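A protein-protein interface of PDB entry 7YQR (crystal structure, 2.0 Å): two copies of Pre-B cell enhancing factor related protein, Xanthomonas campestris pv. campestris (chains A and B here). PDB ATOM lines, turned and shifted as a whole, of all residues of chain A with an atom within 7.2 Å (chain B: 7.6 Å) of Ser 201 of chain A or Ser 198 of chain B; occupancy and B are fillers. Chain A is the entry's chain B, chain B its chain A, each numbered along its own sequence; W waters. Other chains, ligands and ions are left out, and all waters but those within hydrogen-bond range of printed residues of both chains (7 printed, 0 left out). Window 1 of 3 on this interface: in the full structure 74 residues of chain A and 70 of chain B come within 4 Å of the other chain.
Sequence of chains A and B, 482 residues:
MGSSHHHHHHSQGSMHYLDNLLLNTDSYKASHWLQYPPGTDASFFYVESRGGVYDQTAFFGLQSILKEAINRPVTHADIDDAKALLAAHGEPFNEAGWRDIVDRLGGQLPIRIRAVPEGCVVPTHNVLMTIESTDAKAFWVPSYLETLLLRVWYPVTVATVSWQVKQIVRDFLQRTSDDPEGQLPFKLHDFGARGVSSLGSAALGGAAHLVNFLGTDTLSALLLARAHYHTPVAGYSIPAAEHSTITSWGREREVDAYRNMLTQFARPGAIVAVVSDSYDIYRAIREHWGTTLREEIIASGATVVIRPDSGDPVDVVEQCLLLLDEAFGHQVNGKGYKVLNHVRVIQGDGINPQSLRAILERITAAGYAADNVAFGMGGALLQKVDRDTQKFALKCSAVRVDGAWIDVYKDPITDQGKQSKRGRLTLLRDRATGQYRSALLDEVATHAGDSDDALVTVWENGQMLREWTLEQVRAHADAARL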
ATOM      1  N   ARG A 151     -17.418   3.038   4.287  1.00  0.00           N
ATOM      2  CA  ARG A 151     -18.252   2.259   3.375  1.00  0.00           C
ATOM      3  C   ARG A 151     -17.432   1.414   2.395  1.00  0.00           C
ATOM      4  O   ARG A 151     -18.022   0.651   1.630  1.00  0.00           O
ATOM      5  CB  ARG A 151     -19.203   3.178   2.607  1.00  0.00           C
ATOM      6  CG  ARG A 151     -20.312   3.809   3.482  1.00  0.00           C
ATOM      7  CD  ARG A 151     -21.448   4.394   2.629  1.00  0.00           C
ATOM      8  NE  ARG A 151     -21.061   5.636   1.960  1.00  0.00           N
ATOM      9  CZ  ARG A 151     -21.467   6.849   2.338  1.00  0.00           C
ATOM     10  NH1 ARG A 151     -22.279   6.984   3.382  1.00  0.00           N
ATOM     11  NH2 ARG A 151     -21.070   7.927   1.675  1.00  0.00           N
ATOM     12  N   TRP A 153     -16.121  -1.022   3.346  1.00  0.00           N
ATOM     13  CA  TRP A 153     -16.507  -2.357   3.808  1.00  0.00           C
ATOM     14  C   TRP A 153     -17.312  -3.092   2.743  1.00  0.00           C
ATOM     15  O   TRP A 153     -17.184  -4.315   2.601  1.00  0.00           O
ATOM     16  CB  TRP A 153     -17.312  -2.291   5.127  1.00  0.00           C
ATOM     17  CG  TRP A 153     -18.756  -1.814   4.959  1.00  0.00           C
ATOM     18  CD1 TRP A 153     -19.250  -0.559   5.237  1.00  0.00           C
ATOM     19  CD2 TRP A 153     -19.877  -2.585   4.485  1.00  0.00           C
ATOM     20  NE1 TRP A 153     -20.600  -0.505   4.936  1.00  0.00           N
ATOM     21  CE2 TRP A 153     -21.004  -1.736   4.483  1.00  0.00           C
ATOM     22  CE3 TRP A 153     -20.036  -3.913   4.070  1.00  0.00           C
ATOM     23  CZ2 TRP A 153     -22.258  -2.167   4.066  1.00  0.00           C
ATOM     24  CZ3 TRP A 153     -21.284  -4.337   3.646  1.00  0.00           C
ATOM     25  CH2 TRP A 153     -22.379  -3.465   3.650  1.00  0.00           C
ATOM     26  N   TYR A 154     -18.133  -2.366   1.967  1.00  0.00           N
ATOM     27  CA  TYR A 154     -19.058  -3.042   1.055  1.00  0.00           C
ATOM     28  C   TYR A 154     -18.341  -3.665  -0.141  1.00  0.00           C
ATOM     29  O   TYR A 154     -18.479  -4.881  -0.354  1.00  0.00           O
ATOM     30  CB  TYR A 154     -20.172  -2.085   0.621  1.00  0.00           C
ATOM     31  CG  TYR A 154     -21.086  -2.716  -0.405  1.00  0.00           C
ATOM     32  CD1 TYR A 154     -21.835  -3.838  -0.088  1.00  0.00           C
ATOM     33  CD2 TYR A 154     -21.199  -2.192  -1.687  1.00  0.00           C
ATOM     34  CE1 TYR A 154     -22.664  -4.430  -1.030  1.00  0.00           C
ATOM     35  CE2 TYR A 154     -22.031  -2.769  -2.628  1.00  0.00           C
ATOM     36  CZ  TYR A 154     -22.763  -3.881  -2.284  1.00  0.00           C
ATOM     37  OH  TYR A 154     -23.582  -4.444  -3.208  1.00  0.00           O
ATOM     38  N   VAL A 158     -18.082  -7.787  -0.685  1.00  0.00           N
ATOM     39  CA  VAL A 158     -18.601  -8.481  -1.860  1.00  0.00           C
ATOM     40  C   VAL A 158     -17.459  -9.157  -2.623  1.00  0.00           C
ATOM     41  O   VAL A 158     -17.585 -10.306  -3.068  1.00  0.00           O
ATOM     42  CB  VAL A 158     -19.396  -7.519  -2.756  1.00  0.00           C
ATOM     43  CG1 VAL A 158     -19.812  -8.221  -4.046  1.00  0.00           C
ATOM     44  CG2 VAL A 158     -20.681  -7.020  -2.013  1.00  0.00           C
ATOM     45  N   VAL A 196     -30.510  -5.470  -4.978  1.00  0.00           N
ATOM     46  CA  VAL A 196     -29.593  -4.632  -4.214  1.00  0.00           C
ATOM     47  C   VAL A 196     -30.281  -3.288  -3.964  1.00  0.00           C
ATOM     48  O   VAL A 196     -31.269  -2.937  -4.621  1.00  0.00           O
ATOM     49  CB  VAL A 196     -28.242  -4.484  -4.962  1.00  0.00           C
ATOM     50  CG1 VAL A 196     -28.430  -3.684  -6.248  1.00  0.00           C
ATOM     51  CG2 VAL A 196     -27.173  -3.904  -4.079  1.00  0.00           C
ATOM     52  N   SER A 197     -29.779  -2.536  -2.978  1.00  0.00           N
ATOM     53  CA  SER A 197     -30.574  -1.414  -2.455  1.00  0.00           C
ATOM     54  C   SER A 197     -30.566  -0.164  -3.334  1.00  0.00           C
ATOM     55  O   SER A 197     -31.420   0.711  -3.134  1.00  0.00           O
ATOM     56  CB  SER A 197     -30.108  -1.036  -1.045  1.00  0.00           C
ATOM     57  OG  SER A 197     -28.683  -0.852  -0.985  1.00  0.00           O
ATOM     58  N   SER A 198     -29.652  -0.040  -4.301  1.00  0.00           N
ATOM     59  CA  SER A 198     -29.632   1.158  -5.133  1.00  0.00           C
ATOM     60  C   SER A 198     -28.761   0.925  -6.356  1.00  0.00           C
ATOM     61  O   SER A 198     -27.980  -0.027  -6.421  1.00  0.00           O
ATOM     62  CB  SER A 198     -29.113   2.374  -4.365  1.00  0.00           C
ATOM     63  OG  SER A 198     -27.732   2.214  -4.035  1.00  0.00           O
ATOM     64  N   LEU A 199     -28.876   1.857  -7.300  1.00  0.00           N
ATOM     65  CA  LEU A 199     -28.087   1.819  -8.526  1.00  0.00           C
ATOM     66  C   LEU A 199     -26.595   1.917  -8.227  1.00  0.00           C
ATOM     67  O   LEU A 199     -25.783   1.205  -8.835  1.00  0.00           O
ATOM     68  CB  LEU A 199     -28.534   2.958  -9.441  1.00  0.00           C
ATOM     69  CG  LEU A 199     -27.730   3.227 -10.709  1.00  0.00           C
ATOM     70  CD1 LEU A 199     -27.635   1.951 -11.535  1.00  0.00           C
ATOM     71  CD2 LEU A 199     -28.383   4.354 -11.498  1.00  0.00           C
ATOM     72  N   GLY A 200     -26.221   2.792  -7.288  1.00  0.00           N
ATOM     73  CA  GLY A 200     -24.821   2.916  -6.908  1.00  0.00           C
ATOM     74  C   GLY A 200     -24.272   1.657  -6.263  1.00  0.00           C
ATOM     75  O   GLY A 200     -23.130   1.258  -6.520  1.00  0.00           O
ATOM     76  N   SER A 201     -25.071   1.015  -5.413  1.00  0.00           N
ATOM     77  CA  SER A 201     -24.627  -0.244  -4.822  1.00  0.00           C
ATOM     78  C   SER A 201     -24.526  -1.336  -5.877  1.00  0.00           C
ATOM     79  O   SER A 201     -23.584  -2.140  -5.853  1.00  0.00           O
ATOM     80  CB  SER A 201     -25.568  -0.665  -3.701  1.00  0.00           C
ATOM     81  OG  SER A 201     -25.507   0.249  -2.626  1.00  0.00           O
ATOM     82  N   ALA A 202     -25.497  -1.386  -6.800  1.00  0.00           N
ATOM     83  CA  ALA A 202     -25.422  -2.340  -7.899  1.00  0.00           C
ATOM     84  C   ALA A 202     -24.094  -2.204  -8.634  1.00  0.00           C
ATOM     85  O   ALA A 202     -23.409  -3.199  -8.904  1.00  0.00           O
ATOM     86  CB  ALA A 202     -26.590  -2.127  -8.875  1.00  0.00           C
ATOM     87  N   ALA A 203     -23.722  -0.963  -8.962  1.00  0.00           N
ATOM     88  CA  ALA A 203     -22.547  -0.706  -9.785  1.00  0.00           C
ATOM     89  C   ALA A 203     -21.262  -1.128  -9.080  1.00  0.00           C
ATOM     90  O   ALA A 203     -20.407  -1.790  -9.680  1.00  0.00           O
ATOM     91  CB  ALA A 203     -22.493   0.777 -10.162  1.00  0.00           C
ATOM     92  N   LEU A 204     -21.112  -0.752  -7.803  1.00  0.00           N
ATOM     93  CA  LEU A 204     -19.881  -0.998  -7.057  1.00  0.00           C
ATOM     94  C   LEU A 204     -19.805  -2.431  -6.544  1.00  0.00           C
ATOM     95  O   LEU A 204     -18.747  -3.065  -6.616  1.00  0.00           O
ATOM     96  CB  LEU A 204     -19.784  -0.008  -5.886  1.00  0.00           C
ATOM     97  CG  LEU A 204     -18.562  -0.074  -4.961  1.00  0.00           C
ATOM     98  CD1 LEU A 204     -17.225  -0.091  -5.748  1.00  0.00           C
ATOM     99  CD2 LEU A 204     -18.568   1.092  -3.965  1.00  0.00           C
ATOM    100  N   GLY A 205     -20.910  -2.957  -6.007  1.00  0.00           N
ATOM    101  CA  GLY A 205     -20.928  -4.354  -5.609  1.00  0.00           C
ATOM    102  C   GLY A 205     -20.755  -5.277  -6.801  1.00  0.00           C
ATOM    103  O   GLY A 205     -20.033  -6.274  -6.730  1.00  0.00           O
ATOM    104  N   GLY A 206     -21.404  -4.943  -7.920  1.00  0.00           N
ATOM    105  CA  GLY A 206     -21.234  -5.729  -9.125  1.00  0.00           C
ATOM    106  C   GLY A 206     -19.790  -5.735  -9.607  1.00  0.00           C
ATOM    107  O   GLY A 206     -19.284  -6.763 -10.056  1.00  0.00           O
ATOM    108  N   ALA A 207     -19.116  -4.586  -9.534  1.00  0.00           N
ATOM    109  CA  ALA A 207     -17.707  -4.535  -9.931  1.00  0.00           C
ATOM    110  C   ALA A 207     -16.843  -5.354  -8.989  1.00  0.00           C
ATOM    111  O   ALA A 207     -15.832  -5.941  -9.410  1.00  0.00           O
ATOM    112  CB  ALA A 207     -17.220  -3.085  -9.980  1.00  0.00           C
ATOM    113  N   THR A 218     -25.231  -7.617 -14.376  1.00  0.00           N
ATOM    114  CA  THR A 218     -25.343  -6.311 -13.734  1.00  0.00           C
ATOM    115  C   THR A 218     -24.629  -5.289 -14.605  1.00  0.00           C
ATOM    116  O   THR A 218     -23.440  -5.019 -14.435  1.00  0.00           O
ATOM    117  CB  THR A 218     -24.780  -6.354 -12.324  1.00  0.00           C
ATOM    118  OG1 THR A 218     -25.509  -7.319 -11.553  1.00  0.00           O
ATOM    119  CG2 THR A 218     -24.911  -4.991 -11.670  1.00  0.00           C
ATOM    120  N   SER A 220     -24.757  -2.145 -14.661  1.00  0.00           N
ATOM    121  CA  SER A 220     -24.182  -1.033 -13.910  1.00  0.00           C
ATOM    122  C   SER A 220     -22.731  -1.281 -13.548  1.00  0.00           C
ATOM    123  O   SER A 220     -21.952  -0.327 -13.441  1.00  0.00           O
ATOM    124  CB  SER A 220     -25.012  -0.748 -12.643  1.00  0.00           C
ATOM    125  OG  SER A 220     -26.387  -0.633 -12.996  1.00  0.00           O
ATOM    126  N   LEU A 224     -19.359   1.178 -14.109  1.00  0.00           N
ATOM    127  CA  LEU A 224     -18.408   1.576 -13.078  1.00  0.00           C
ATOM    128  C   LEU A 224     -16.984   1.146 -13.434  1.00  0.00           C
ATOM    129  O   LEU A 224     -16.042   1.928 -13.269  1.00  0.00           O
ATOM    130  CB  LEU A 224     -18.816   0.990 -11.727  1.00  0.00           C
ATOM    131  CG  LEU A 224     -18.044   1.595 -10.552  1.00  0.00           C
ATOM    132  CD1 LEU A 224     -18.939   1.854  -9.334  1.00  0.00           C
ATOM    133  CD2 LEU A 224     -16.866   0.683 -10.159  1.00  0.00           C
ATOM    134  N   LEU A 382     -24.929  -9.404  -3.552  1.00  0.00           N
ATOM    135  CA  LEU A 382     -24.843  -7.950  -3.551  1.00  0.00           C
ATOM    136  C   LEU A 382     -25.534  -7.291  -2.367  1.00  0.00           C
ATOM    137  O   LEU A 382     -25.206  -6.144  -2.046  1.00  0.00           O
ATOM    138  CB  LEU A 382     -25.435  -7.371  -4.837  1.00  0.00           C
ATOM    139  CG  LEU A 382     -24.811  -7.825  -6.153  1.00  0.00           C
ATOM    140  CD1 LEU A 382     -25.386  -6.985  -7.295  1.00  0.00           C
ATOM    141  CD2 LEU A 382     -23.289  -7.716  -6.098  1.00  0.00           C
ATOM    142  N   GLN A 383     -26.439  -7.980  -1.692  1.00  0.00           N
ATOM    143  CA  GLN A 383     -27.245  -7.316  -0.676  1.00  0.00           C
ATOM    144  C   GLN A 383     -27.118  -7.930   0.707  1.00  0.00           C
ATOM    145  O   GLN A 383     -27.098  -7.195   1.706  1.00  0.00           O
ATOM    146  CB  GLN A 383     -28.729  -7.301  -1.126  1.00  0.00           C
ATOM    147  CG  GLN A 383     -29.655  -6.496  -0.179  1.00  0.00           C
ATOM    148  CD  GLN A 383     -29.225  -5.047   0.023  1.00  0.00           C
ATOM    149  OE1 GLN A 383     -28.773  -4.364  -0.906  1.00  0.00           O
ATOM    150  NE2 GLN A 383     -29.397  -4.561   1.248  1.00  0.00           N
ATOM    151  N   TYR B  17     -21.421   8.765 -15.086  1.00  0.00           N
ATOM    152  CA  TYR B  17     -21.168   7.493 -15.756  1.00  0.00           C
ATOM    153  C   TYR B  17     -22.361   6.537 -15.698  1.00  0.00           C
ATOM    154  O   TYR B  17     -22.404   5.576 -16.473  1.00  0.00           O
ATOM    155  CB  TYR B  17     -19.910   6.832 -15.169  1.00  0.00           C
ATOM    156  CG  TYR B  17     -20.038   6.334 -13.737  1.00  0.00           C
ATOM    157  CD1 TYR B  17     -19.929   7.203 -12.662  1.00  0.00           C
ATOM    158  CD2 TYR B  17     -20.275   4.994 -13.469  1.00  0.00           C
ATOM    159  CE1 TYR B  17     -20.049   6.751 -11.355  1.00  0.00           C
ATOM    160  CE2 TYR B  17     -20.397   4.529 -12.155  1.00  0.00           C
ATOM    161  CZ  TYR B  17     -20.296   5.417 -11.113  1.00  0.00           C
ATOM    162  OH  TYR B  17     -20.434   4.977  -9.815  1.00  0.00           O
ATOM    163  N   LEU B  18     -23.335   6.770 -14.817  1.00  0.00           N
ATOM    164  CA  LEU B  18     -24.542   5.946 -14.773  1.00  0.00           C
ATOM    165  C   LEU B  18     -25.746   6.601 -15.436  1.00  0.00           C
ATOM    166  O   LEU B  18     -26.863   6.090 -15.303  1.00  0.00           O
ATOM    167  CB  LEU B  18     -24.899   5.590 -13.330  1.00  0.00           C
ATOM    168  CG  LEU B  18     -23.778   4.835 -12.607  1.00  0.00           C
ATOM    169  CD1 LEU B  18     -23.961   4.888 -11.097  1.00  0.00           C
ATOM    170  CD2 LEU B  18     -23.697   3.398 -13.140  1.00  0.00           C
ATOM    171  N   ARG B 151     -36.335  -2.274  -7.276  1.00  0.00           N
ATOM    172  CA  ARG B 151     -35.537  -1.810  -6.141  1.00  0.00           C
ATOM    173  C   ARG B 151     -36.330  -0.892  -5.191  1.00  0.00           C
ATOM    174  O   ARG B 151     -35.802  -0.473  -4.148  1.00  0.00           O
ATOM    175  CB  ARG B 151     -34.273  -1.109  -6.645  1.00  0.00           C
ATOM    176  CG  ARG B 151     -33.233  -2.077  -7.270  1.00  0.00           C
ATOM    177  CD  ARG B 151     -31.852  -1.416  -7.413  1.00  0.00           C
ATOM    178  NE  ARG B 151     -31.852  -0.427  -8.497  1.00  0.00           N
ATOM    179  CZ  ARG B 151     -31.197  -0.580  -9.642  1.00  0.00           C
ATOM    180  NH1 ARG B 151     -30.492  -1.689  -9.856  1.00  0.00           N
ATOM    181  NH2 ARG B 151     -31.230   0.374 -10.557  1.00  0.00           N
ATOM    182  N   TYR B 154     -36.426  -1.561  -1.419  1.00  0.00           N
ATOM    183  CA  TYR B 154     -35.498  -1.133  -0.380  1.00  0.00           C
ATOM    184  C   TYR B 154     -36.100  -0.014   0.472  1.00  0.00           C
ATOM    185  O   TYR B 154     -36.177  -0.161   1.700  1.00  0.00           O
ATOM    186  CB  TYR B 154     -34.148  -0.708  -0.981  1.00  0.00           C
ATOM    187  CG  TYR B 154     -33.223  -0.085   0.024  1.00  0.00           C
ATOM    188  CD1 TYR B 154     -32.763  -0.819   1.105  1.00  0.00           C
ATOM    189  CD2 TYR B 154     -32.793   1.235  -0.109  1.00  0.00           C
ATOM    190  CE1 TYR B 154     -31.920  -0.271   2.037  1.00  0.00           C
ATOM    191  CE2 TYR B 154     -31.922   1.800   0.837  1.00  0.00           C
ATOM    192  CZ  TYR B 154     -31.493   1.033   1.900  1.00  0.00           C
ATOM    193  OH  TYR B 154     -30.632   1.564   2.857  1.00  0.00           O
ATOM    194  N   GLY B 192     -26.857   4.979  10.540  1.00  0.00           N
ATOM    195  CA  GLY B 192     -26.401   3.978   9.597  1.00  0.00           C
ATOM    196  C   GLY B 192     -25.571   4.402   8.397  1.00  0.00           C
ATOM    197  O   GLY B 192     -25.239   3.531   7.588  1.00  0.00           O
ATOM    198  N   ALA B 193     -25.199   5.679   8.257  1.00  0.00           N
ATOM    199  CA  ALA B 193     -24.569   6.142   7.021  1.00  0.00           C
ATOM    200  C   ALA B 193     -23.241   5.412   6.729  1.00  0.00           C
ATOM    201  O   ALA B 193     -22.945   5.095   5.568  1.00  0.00           O
ATOM    202  CB  ALA B 193     -24.359   7.652   7.089  1.00  0.00           C
ATOM    203  N   ARG B 194     -22.447   5.115   7.764  1.00  0.00           N
ATOM    204  CA  ARG B 194     -21.198   4.372   7.562  1.00  0.00           C
ATOM    205  C   ARG B 194     -21.411   2.876   7.339  1.00  0.00           C
ATOM    206  O   ARG B 194     -20.497   2.204   6.841  1.00  0.00           O
ATOM    207  CB  ARG B 194     -20.263   4.556   8.766  1.00  0.00           C
ATOM    208  CG  ARG B 194     -20.617   3.666   9.953  1.00  0.00           C
ATOM    209  CD  ARG B 194     -19.938   4.099  11.256  1.00  0.00           C
ATOM    210  NE  ARG B 194     -20.128   5.521  11.529  1.00  0.00           N
ATOM    211  CZ  ARG B 194     -19.440   6.196  12.444  1.00  0.00           C
ATOM    212  NH1 ARG B 194     -18.536   5.574  13.180  1.00  0.00           N
ATOM    213  NH2 ARG B 194     -19.654   7.493  12.624  1.00  0.00           N
ATOM    214  N   GLY B 195     -22.574   2.337   7.708  1.00  0.00           N
ATOM    215  CA  GLY B 195     -22.869   0.918   7.672  1.00  0.00           C
ATOM    216  C   GLY B 195     -23.686   0.454   6.485  1.00  0.00           C
ATOM    217  O   GLY B 195     -24.033  -0.732   6.421  1.00  0.00           O
ATOM    218  N   VAL B 196     -23.997   1.340   5.548  1.00  0.00           N
ATOM    219  CA  VAL B 196     -24.789   1.014   4.378  1.00  0.00           C
ATOM    220  C   VAL B 196     -23.870   0.949   3.159  1.00  0.00           C
ATOM    221  O   VAL B 196     -22.728   1.402   3.189  1.00  0.00           O
ATOM    222  CB  VAL B 196     -25.956   2.030   4.192  1.00  0.00           C
ATOM    223  CG1 VAL B 196     -25.427   3.415   3.819  1.00  0.00           C
ATOM    224  CG2 VAL B 196     -26.987   1.520   3.192  1.00  0.00           C
ATOM    225  N   SER B 197     -24.375   0.376   2.060  1.00  0.00           N
ATOM    226  CA  SER B 197     -23.504  -0.061   0.971  1.00  0.00           C
ATOM    227  C   SER B 197     -23.103   1.052   0.008  1.00  0.00           C
ATOM    228  O   SER B 197     -22.142   0.866  -0.741  1.00  0.00           O
ATOM    229  CB  SER B 197     -24.169  -1.222   0.214  1.00  0.00           C
ATOM    230  OG  SER B 197     -25.487  -0.903  -0.224  1.00  0.00           O
ATOM    231  N   SER B 198     -23.780   2.199   0.017  1.00  0.00           N
ATOM    232  CA  SER B 198     -23.406   3.294  -0.874  1.00  0.00           C
ATOM    233  C   SER B 198     -24.060   4.587  -0.401  1.00  0.00           C
ATOM    234  O   SER B 198     -24.966   4.583   0.439  1.00  0.00           O
ATOM    235  CB  SER B 198     -23.806   3.005  -2.331  1.00  0.00           C
ATOM    236  OG  SER B 198     -25.212   3.055  -2.507  1.00  0.00           O
ATOM    237  N   LEU B 199     -23.595   5.694  -0.990  1.00  0.00           N
ATOM    238  CA  LEU B 199     -24.160   7.014  -0.725  1.00  0.00           C
ATOM    239  C   LEU B 199     -25.627   7.095  -1.153  1.00  0.00           C
ATOM    240  O   LEU B 199     -26.460   7.647  -0.426  1.00  0.00           O
ATOM    241  CB  LEU B 199     -23.330   8.074  -1.454  1.00  0.00           C
ATOM    242  CG  LEU B 199     -23.816   9.520  -1.555  1.00  0.00           C
ATOM    243  CD1 LEU B 199     -23.966  10.134  -0.151  1.00  0.00           C
ATOM    244  CD2 LEU B 199     -22.821  10.331  -2.389  1.00  0.00           C
ATOM    245  N   GLY B 200     -25.961   6.589  -2.346  1.00  0.00           N
ATOM    246  CA  GLY B 200     -27.353   6.613  -2.775  1.00  0.00           C
ATOM    247  C   GLY B 200     -28.271   5.808  -1.870  1.00  0.00           C
ATOM    248  O   GLY B 200     -29.424   6.192  -1.641  1.00  0.00           O
ATOM    249  N   SER B 201     -27.779   4.688  -1.345  1.00  0.00           N
ATOM    250  CA  SER B 201     -28.567   3.889  -0.414  1.00  0.00           C
ATOM    251  C   SER B 201     -28.723   4.602   0.924  1.00  0.00           C
ATOM    252  O   SER B 201     -29.796   4.544   1.541  1.00  0.00           O
ATOM    253  CB  SER B 201     -27.919   2.516  -0.225  1.00  0.00           C
ATOM    254  OG  SER B 201     -28.101   1.730  -1.391  1.00  0.00           O
ATOM    255  N   ALA B 202     -27.658   5.260   1.393  1.00  0.00           N
ATOM    256  CA  ALA B 202     -27.747   6.077   2.601  1.00  0.00           C
ATOM    257  C   ALA B 202     -28.812   7.154   2.456  1.00  0.00           C
ATOM    258  O   ALA B 202     -29.607   7.371   3.370  1.00  0.00           O
ATOM    259  CB  ALA B 202     -26.397   6.722   2.906  1.00  0.00           C
ATOM    260  N   ALA B 203     -28.835   7.838   1.311  1.00  0.00           N
ATOM    261  CA  ALA B 203     -29.800   8.907   1.098  1.00  0.00           C
ATOM    262  C   ALA B 203     -31.228   8.367   1.072  1.00  0.00           C
ATOM    263  O   ALA B 203     -32.109   8.889   1.759  1.00  0.00           O
ATOM    264  CB  ALA B 203     -29.475   9.652  -0.196  1.00  0.00           C
ATOM    265  N   LEU B 204     -31.476   7.311   0.296  1.00  0.00           N
ATOM    266  CA  LEU B 204     -32.842   6.827   0.125  1.00  0.00           C
ATOM    267  C   LEU B 204     -33.312   6.020   1.337  1.00  0.00           C
ATOM    268  O   LEU B 204     -34.425   6.233   1.841  1.00  0.00           O
ATOM    269  CB  LEU B 204     -32.935   6.008  -1.172  1.00  0.00           C
ATOM    270  CG  LEU B 204     -34.319   5.442  -1.506  1.00  0.00           C
ATOM    271  CD1 LEU B 204     -35.359   6.560  -1.578  1.00  0.00           C
ATOM    272  CD2 LEU B 204     -34.280   4.660  -2.825  1.00  0.00           C
ATOM    273  N   SER B 220     -27.118  12.666   4.194  1.00  0.00           N
ATOM    274  CA  SER B 220     -27.545  12.369   2.832  1.00  0.00           C
ATOM    275  C   SER B 220     -29.062  12.253   2.719  1.00  0.00           C
ATOM    276  O   SER B 220     -29.628  12.500   1.645  1.00  0.00           O
ATOM    277  CB  SER B 220     -26.872  11.073   2.344  1.00  0.00           C
ATOM    278  OG  SER B 220     -25.464  11.174   2.511  1.00  0.00           O
ATOM    279  N   LEU B 382     -30.447   0.350   7.944  1.00  0.00           N
ATOM    280  CA  LEU B 382     -30.179   0.685   6.547  1.00  0.00           C
ATOM    281  C   LEU B 382     -29.630  -0.479   5.713  1.00  0.00           C
ATOM    282  O   LEU B 382     -29.732  -0.438   4.480  1.00  0.00           O
ATOM    283  CB  LEU B 382     -29.191   1.861   6.471  1.00  0.00           C
ATOM    284  CG  LEU B 382     -29.662   3.193   7.103  1.00  0.00           C
ATOM    285  CD1 LEU B 382     -28.778   4.357   6.658  1.00  0.00           C
ATOM    286  CD2 LEU B 382     -31.118   3.470   6.752  1.00  0.00           C
ATOM    287  N   GLN B 383     -29.051  -1.498   6.324  1.00  0.00           N
ATOM    288  CA  GLN B 383     -28.323  -2.488   5.517  1.00  0.00           C
ATOM    289  C   GLN B 383     -28.802  -3.920   5.699  1.00  0.00           C
ATOM    290  O   GLN B 383     -28.806  -4.686   4.721  1.00  0.00           O
ATOM    291  CB  GLN B 383     -26.822  -2.411   5.822  1.00  0.00           C
ATOM    292  CG  GLN B 383     -25.906  -3.342   4.945  1.00  0.00           C
ATOM    293  CD  GLN B 383     -26.024  -3.060   3.469  1.00  0.00           C
ATOM    294  OE1 GLN B 383     -26.218  -1.916   3.060  1.00  0.00           O
ATOM    295  NE2 GLN B 383     -25.898  -4.104   2.649  1.00  0.00           N
HETATM  296  O   HOH W   1     -28.408  -1.626   1.651  1.00  0.00           O
HETATM  297  O   HOH W   2     -29.086  -1.479 -12.406  1.00  0.00           O
HETATM  298  O   HOH W   3     -23.259   9.884   3.504  1.00  0.00           O
HETATM  299  O   HOH W   4     -28.151  -7.311   4.422  1.00  0.00           O
HETATM  300  O   HOH W   5     -33.825   1.542  -4.058  1.00  0.00           O
HETATM  301  O   HOH W   6     -19.456   1.321  -0.703  1.00  0.00           O
HETATM  302  O   HOH W   7     -26.165  -3.684  -0.412  1.00  0.00           O
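O of Arg 194 of chain B lies within hydrogen-bond range of NE1 of Trp 153 of chain A.
The backbone carbonyl oxygen (O) of Val 196 of chain B is in hydrogen-bond range of the indole nitrogen (NE1) of Trp 153 of chain A (3.3 Å).
OG of Ser 197 of chain B sits at hydrogen-bond distance from OG of Ser 197 of chain A, at 3.3 Å.
The side-chain hydroxyl of Ser 201 of chain A is in hydrogen-bond range of the side-chain hydroxyl of Ser 197 of chain B, 2.7 Å away.
The side-chain hydroxyl of Ser 198 of chain A lies within hydrogen-bond range of the side-chain hydroxyl of Ser 198 of chain B (3.1 Å).
The side-chain hydroxyl (OG) of Ser 197 of chain A lies within hydrogen-bond range of the side-chain hydroxyl (OG) of Ser 201 of chain B, at 2.7 Å.
The side-chain amide nitrogen (NE2) of Gln 383 of chain B is in hydrogen-bond range of the backbone carbonyl oxygen (O) of Gln 383 of chain A (3.4 Å).
Arg 151 of chain B touches Val 196 of chain A.
Arg 151 of chain B touches Ser 198 of chain A.
Leu 199 of chain A touches Arg 151 of chain B (CB to NH2, 3.9 Å).
Leu 224 of chain A touches Tyr 17 of chain B (CD1 to OH, 3.5 Å).
Gln 383 of chain B touches its own counterpart, Gln 383 of chain A.
Of the 24 pairs that touch across the chains among the printed residues, 16 have their exchanged pair printed and touching as well.
Of the printed residues of chain B, Tyr 154 of chain A touches Ser 197.
No residue of chain B comes within 4 Å of Gly 200 of chain A.
Of chain A, only Arg 151 (3.96 Å), Ser 198 (3.1 Å) and Ser 201 (2.8 Å) come within 4 Å of Ser 198 of chain B.
Ala 203 of chain B touches none of the printed residues of chain A.
Leu 204 of chain B touches none of the printed residues of chain A.
The nearest residue of chain B that does not touch Ser 201 of chain A is Leu 199 of chain B (6.0 Å).
The backbone carbonyl oxygen (O) of Leu 382 of chain A lies within hydrogen-bond range of the side-chain hydroxyl (OH) of Tyr 154 of chain A, at 2.6 Å.
Hydrophobic or aromatic side chains of chain B within 4 Å of the printed part of chain A: Tyr 17, Tyr 154 and Leu 199.
Hydrophobic or aromatic side chains of chain A within 4 Å of the printed part of chain B: Trp 153, Tyr 154, Leu 199 and Leu 224.
Among the printed residues, no Asp or Glu carboxylate lies within 4 Å of a Lys or Arg side-chain nitrogen of the other chain.
Water W4 lies within hydrogen-bond range of the backbone carbonyl oxygen (O) of Gln 383 of chain B and the backbone carbonyl oxygen (O) of Gln 383 of chain A.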
